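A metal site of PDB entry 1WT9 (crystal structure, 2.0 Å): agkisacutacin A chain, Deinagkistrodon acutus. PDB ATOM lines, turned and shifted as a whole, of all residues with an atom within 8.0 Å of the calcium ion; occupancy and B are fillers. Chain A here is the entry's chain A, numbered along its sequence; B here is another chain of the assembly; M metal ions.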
ATOM      1  N   TYR A   9       1.930  16.879  -8.094  1.00  0.00           N
ATOM      2  CA  TYR A   9       0.574  17.413  -8.101  1.00  0.00           C
ATOM      3  C   TYR A   9       0.434  18.207  -9.396  1.00  0.00           C
ATOM      4  O   TYR A   9       1.212  19.126  -9.641  1.00  0.00           O
ATOM      5  CB  TYR A   9       0.337  18.348  -6.906  1.00  0.00           C
ATOM      6  CG  TYR A   9      -1.007  19.047  -6.943  1.00  0.00           C
ATOM      7  CD1 TYR A   9      -2.181  18.359  -6.616  1.00  0.00           C
ATOM      8  CD2 TYR A   9      -1.114  20.365  -7.385  1.00  0.00           C
ATOM      9  CE1 TYR A   9      -3.439  18.973  -6.717  1.00  0.00           C
ATOM     10  CE2 TYR A   9      -2.368  20.985  -7.494  1.00  0.00           C
ATOM     11  CZ  TYR A   9      -3.516  20.286  -7.162  1.00  0.00           C
ATOM     12  OH  TYR A   9      -4.757  20.895  -7.285  1.00  0.00           O
ATOM     13  N   HIS A  12       3.553  18.968 -11.536  1.00  0.00           N
ATOM     14  CA  HIS A  12       4.678  19.612 -10.862  1.00  0.00           C
ATOM     15  C   HIS A  12       5.177  18.728  -9.728  1.00  0.00           C
ATOM     16  O   HIS A  12       4.475  17.822  -9.288  1.00  0.00           O
ATOM     17  CB  HIS A  12       4.291  20.986 -10.293  1.00  0.00           C
ATOM     18  CG  HIS A  12       4.131  22.036 -11.346  1.00  0.00           C
ATOM     19  ND1 HIS A  12       4.753  21.974 -12.575  1.00  0.00           N
ATOM     20  CD2 HIS A  12       3.449  23.207 -11.330  1.00  0.00           C
ATOM     21  CE1 HIS A  12       4.456  23.046 -13.271  1.00  0.00           C
ATOM     22  NE2 HIS A  12       3.674  23.814 -12.541  1.00  0.00           N
ATOM     23  N   CYS A  13       6.396  19.003  -9.270  1.00  0.00           N
ATOM     24  CA  CYS A  13       7.026  18.236  -8.205  1.00  0.00           C
ATOM     25  C   CYS A  13       7.350  19.159  -7.044  1.00  0.00           C
ATOM     26  O   CYS A  13       7.904  20.248  -7.257  1.00  0.00           O
ATOM     27  CB  CYS A  13       8.305  17.573  -8.720  1.00  0.00           C
ATOM     28  SG  CYS A  13       8.017  16.443 -10.135  1.00  0.00           S
ATOM     29  N   TYR A  14       7.006  18.736  -5.833  1.00  0.00           N
ATOM     30  CA  TYR A  14       7.234  19.553  -4.643  1.00  0.00           C
ATOM     31  C   TYR A  14       8.025  18.815  -3.588  1.00  0.00           C
ATOM     32  O   TYR A  14       8.020  17.583  -3.548  1.00  0.00           O
ATOM     33  CB  TYR A  14       5.905  19.998  -4.048  1.00  0.00           C
ATOM     34  CG  TYR A  14       4.967  20.681  -5.026  1.00  0.00           C
ATOM     35  CD1 TYR A  14       4.324  19.945  -6.023  1.00  0.00           C
ATOM     36  CD2 TYR A  14       4.713  22.039  -4.940  1.00  0.00           C
ATOM     37  CE1 TYR A  14       3.441  20.548  -6.888  1.00  0.00           C
ATOM     38  CE2 TYR A  14       3.829  22.654  -5.810  1.00  0.00           C
ATOM     39  CZ  TYR A  14       3.191  21.903  -6.788  1.00  0.00           C
ATOM     40  OH  TYR A  14       2.308  22.506  -7.653  1.00  0.00           O
ATOM     41  N   LEU A  39      11.280  28.492  -5.239  1.00  0.00           N
ATOM     42  CA  LEU A  39      10.463  28.423  -4.043  1.00  0.00           C
ATOM     43  C   LEU A  39       9.047  28.217  -4.621  1.00  0.00           C
ATOM     44  O   LEU A  39       8.742  28.680  -5.719  1.00  0.00           O
ATOM     45  CB  LEU A  39      10.547  29.731  -3.240  1.00  0.00           C
ATOM     46  CG  LEU A  39      11.742  29.841  -2.289  1.00  0.00           C
ATOM     47  CD1 LEU A  39      11.868  31.258  -1.753  1.00  0.00           C
ATOM     48  CD2 LEU A  39      11.534  28.855  -1.120  1.00  0.00           C
ATOM     49  N   VAL A  40       8.200  27.512  -3.892  1.00  0.00           N
ATOM     50  CA  VAL A  40       6.863  27.229  -4.395  1.00  0.00           C
ATOM     51  C   VAL A  40       6.033  28.445  -4.797  1.00  0.00           C
ATOM     52  O   VAL A  40       6.167  29.522  -4.219  1.00  0.00           O
ATOM     53  CB  VAL A  40       6.037  26.414  -3.358  1.00  0.00           C
ATOM     54  CG1 VAL A  40       5.658  27.301  -2.169  1.00  0.00           C
ATOM     55  CG2 VAL A  40       4.788  25.851  -4.024  1.00  0.00           C
ATOM     56  N   SER A  41       5.189  28.270  -5.820  1.00  0.00           N
ATOM     57  CA  SER A  41       4.274  29.316  -6.266  1.00  0.00           C
ATOM     58  C   SER A  41       2.882  28.714  -6.072  1.00  0.00           C
ATOM     59  O   SER A  41       2.648  27.579  -6.453  1.00  0.00           O
ATOM     60  CB  SER A  41       4.484  29.688  -7.735  1.00  0.00           C
ATOM     61  OG  SER A  41       4.262  28.585  -8.596  1.00  0.00           O
ATOM     62  N   ILE A  42       1.979  29.472  -5.454  1.00  0.00           N
ATOM     63  CA  ILE A  42       0.627  28.989  -5.217  1.00  0.00           C
ATOM     64  C   ILE A  42      -0.273  29.744  -6.196  1.00  0.00           C
ATOM     65  O   ILE A  42      -0.549  30.928  -6.002  1.00  0.00           O
ATOM     66  CB  ILE A  42       0.210  29.244  -3.762  1.00  0.00           C
ATOM     67  CG1 ILE A  42       1.169  28.472  -2.843  1.00  0.00           C
ATOM     68  CG2 ILE A  42      -1.237  28.768  -3.538  1.00  0.00           C
ATOM     69  CD1 ILE A  42       0.975  28.754  -1.359  1.00  0.00           C
ATOM     70  N   GLU A  43      -0.725  29.057  -7.240  1.00  0.00           N
ATOM     71  CA  GLU A  43      -1.544  29.682  -8.265  1.00  0.00           C
ATOM     72  C   GLU A  43      -3.014  29.298  -8.335  1.00  0.00           C
ATOM     73  O   GLU A  43      -3.683  29.630  -9.312  1.00  0.00           O
ATOM     74  CB  GLU A  43      -0.862  29.480  -9.618  1.00  0.00           C
ATOM     75  CG  GLU A  43       0.524  30.106  -9.648  1.00  0.00           C
ATOM     76  CD  GLU A  43       1.298  29.777 -10.901  1.00  0.00           C
ATOM     77  OE1 GLU A  43       0.845  30.163 -12.001  1.00  0.00           O
ATOM     78  OE2 GLU A  43       2.354  29.131 -10.783  1.00  0.00           O
ATOM     79  N   SER A  44      -3.520  28.591  -7.326  1.00  0.00           N
ATOM     80  CA  SER A  44      -4.931  28.200  -7.310  1.00  0.00           C
ATOM     81  C   SER A  44      -5.310  27.577  -5.976  1.00  0.00           C
ATOM     82  O   SER A  44      -4.440  27.169  -5.196  1.00  0.00           O
ATOM     83  CB  SER A  44      -5.243  27.209  -8.433  1.00  0.00           C
ATOM     84  OG  SER A  44      -4.622  25.963  -8.170  1.00  0.00           O
ATOM     85  N   GLU A  47      -3.989  24.005  -5.654  1.00  0.00           N
ATOM     86  CA  GLU A  47      -2.567  23.953  -5.337  1.00  0.00           C
ATOM     87  C   GLU A  47      -2.346  24.349  -3.872  1.00  0.00           C
ATOM     88  O   GLU A  47      -1.593  23.697  -3.160  1.00  0.00           O
ATOM     89  CB  GLU A  47      -1.775  24.860  -6.280  1.00  0.00           C
ATOM     90  CG  GLU A  47      -0.290  24.878  -6.017  1.00  0.00           C
ATOM     91  CD  GLU A  47       0.502  25.480  -7.166  1.00  0.00           C
ATOM     92  OE1 GLU A  47       0.007  26.442  -7.793  1.00  0.00           O
ATOM     93  OE2 GLU A  47       1.614  24.996  -7.440  1.00  0.00           O
ATOM     94  N   ALA A  48      -2.996  25.420  -3.423  1.00  0.00           N
ATOM     95  CA  ALA A  48      -2.867  25.861  -2.035  1.00  0.00           C
ATOM     96  C   ALA A  48      -3.234  24.744  -1.046  1.00  0.00           C
ATOM     97  O   ALA A  48      -2.596  24.591  -0.007  1.00  0.00           O
ATOM     98  CB  ALA A  48      -3.748  27.093  -1.778  1.00  0.00           C
ATOM     99  N   VAL A  51      -0.345  21.968  -1.261  1.00  0.00           N
ATOM    100  CA  VAL A  51       0.891  22.462  -0.631  1.00  0.00           C
ATOM    101  C   VAL A  51       0.708  22.609   0.873  1.00  0.00           C
ATOM    102  O   VAL A  51       1.596  22.262   1.649  1.00  0.00           O
ATOM    103  CB  VAL A  51       1.320  23.807  -1.259  1.00  0.00           C
ATOM    104  CG1 VAL A  51       2.513  24.389  -0.503  1.00  0.00           C
ATOM    105  CG2 VAL A  51       1.657  23.603  -2.717  1.00  0.00           C
ATOM    106  N   GLU A 128       9.643  23.834  -5.672  1.00  0.00           N
ATOM    107  CA  GLU A 128       8.747  23.337  -6.707  1.00  0.00           C
ATOM    108  C   GLU A 128       9.460  23.347  -8.051  1.00  0.00           C
ATOM    109  O   GLU A 128      10.280  24.225  -8.316  1.00  0.00           O
ATOM    110  CB  GLU A 128       7.494  24.218  -6.790  1.00  0.00           C
ATOM    111  CG  GLU A 128       6.525  23.827  -7.904  1.00  0.00           C
ATOM    112  CD  GLU A 128       5.402  24.832  -8.078  1.00  0.00           C
ATOM    113  OE1 GLU A 128       5.395  25.843  -7.353  1.00  0.00           O
ATOM    114  OE2 GLU A 128       4.520  24.624  -8.937  1.00  0.00           O
ATOM    115  N   ALA A 129       9.161  22.356  -8.877  1.00  0.00           N
ATOM    116  CA  ALA A 129       9.726  22.251 -10.221  1.00  0.00           C
ATOM    117  C   ALA A 129       8.668  21.630 -11.117  1.00  0.00           C
ATOM    118  O   ALA A 129       8.475  22.073 -12.240  1.00  0.00           O
ATOM    119  CB  ALA A 129      10.977  21.399 -10.222  1.00  0.00           C
ATOM    120  OXT ALA A 129       8.040  20.644 -10.669  1.00  0.00           O
ATOM    121  N   TRP B  79       6.303  36.288  -8.409  1.00  0.00           N
ATOM    122  CA  TRP B  79       6.649  34.924  -8.015  1.00  0.00           C
ATOM    123  C   TRP B  79       8.062  34.731  -8.552  1.00  0.00           C
ATOM    124  O   TRP B  79       8.366  35.210  -9.644  1.00  0.00           O
ATOM    125  CB  TRP B  79       5.716  33.910  -8.660  1.00  0.00           C
ATOM    126  CG  TRP B  79       4.335  33.847  -8.069  1.00  0.00           C
ATOM    127  CD1 TRP B  79       3.170  34.207  -8.670  1.00  0.00           C
ATOM    128  CD2 TRP B  79       3.988  33.342  -6.772  1.00  0.00           C
ATOM    129  NE1 TRP B  79       2.113  33.969  -7.828  1.00  0.00           N
ATOM    130  CE2 TRP B  79       2.577  33.440  -6.649  1.00  0.00           C
ATOM    131  CE3 TRP B  79       4.723  32.819  -5.695  1.00  0.00           C
ATOM    132  CZ2 TRP B  79       1.890  33.039  -5.503  1.00  0.00           C
ATOM    133  CZ3 TRP B  79       4.031  32.426  -4.546  1.00  0.00           C
ATOM    134  CH2 TRP B  79       2.627  32.541  -4.460  1.00  0.00           C
ATOM    135  N   ASN B  81       9.323  32.188  -9.771  1.00  0.00           N
ATOM    136  CA  ASN B  81       9.365  31.305 -10.932  1.00  0.00           C
ATOM    137  C   ASN B  81       8.751  32.038 -12.113  1.00  0.00           C
ATOM    138  O   ASN B  81       8.415  31.421 -13.123  1.00  0.00           O
ATOM    139  CB  ASN B  81       8.611  30.013 -10.634  1.00  0.00           C
ATOM    140  CG  ASN B  81       7.108  30.196 -10.663  1.00  0.00           C
ATOM    141  OD1 ASN B  81       6.595  31.294 -10.466  1.00  0.00           O
ATOM    142  ND2 ASN B  81       6.386  29.098 -10.886  1.00  0.00           N
ATOM    143  N   ALA B  83       5.895  33.187 -12.571  1.00  0.00           N
ATOM    144  CA  ALA B  83       4.490  32.932 -12.822  1.00  0.00           C
ATOM    145  C   ALA B  83       3.709  34.218 -12.612  1.00  0.00           C
ATOM    146  O   ALA B  83       4.078  35.056 -11.788  1.00  0.00           O
ATOM    147  CB  ALA B  83       3.963  31.849 -11.895  1.00  0.00           C
HETATM  148 CA    CA M   1       3.074  26.412  -8.356  1.00  0.00          CA
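The side-chain carboxylate (OE1) of Glu 47 is in hydrogen-bond range of the backbone NH (N) of Glu 43, at 2.8 Å. The side-chain carboxylate of Glu 47 lies close to the side-chain hydroxyl of Tyr 14 (2.6 Å). The side-chain hydroxyl of Ser 44 is in hydrogen-bond range of the backbone NH of Glu 47, at 3.3 Å. The side-chain carboxylate of Glu 43 sits close to the side-chain hydroxyl of Ser 41 (3.0 Å). ND2 of Asn 81 of chain B lies close to OG of Ser 41. The side-chain carboxylate of Glu 128 sits close to the side-chain hydroxyl of Tyr 14.
Glu 43 touches the calcium ion. Four residues have an atom within 4 Å of the calcium ion: Ser 41, Glu 43, Glu 47 and Glu 128. Along chain A the residues within 4 Å of the calcium ion span positions 41 to 128.
The calcium ion is bound by OE2 of Glu 47 (2.2 Å), O of Ser 41 (2.3 Å), OE2 of Glu 128 (2.4 Å), OG of Ser 41 (2.5 Å) and OE1 of Glu 128 (2.6 Å). Slightly farther from the calcium ion lies OE1 of Glu 47 (3.1 Å).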
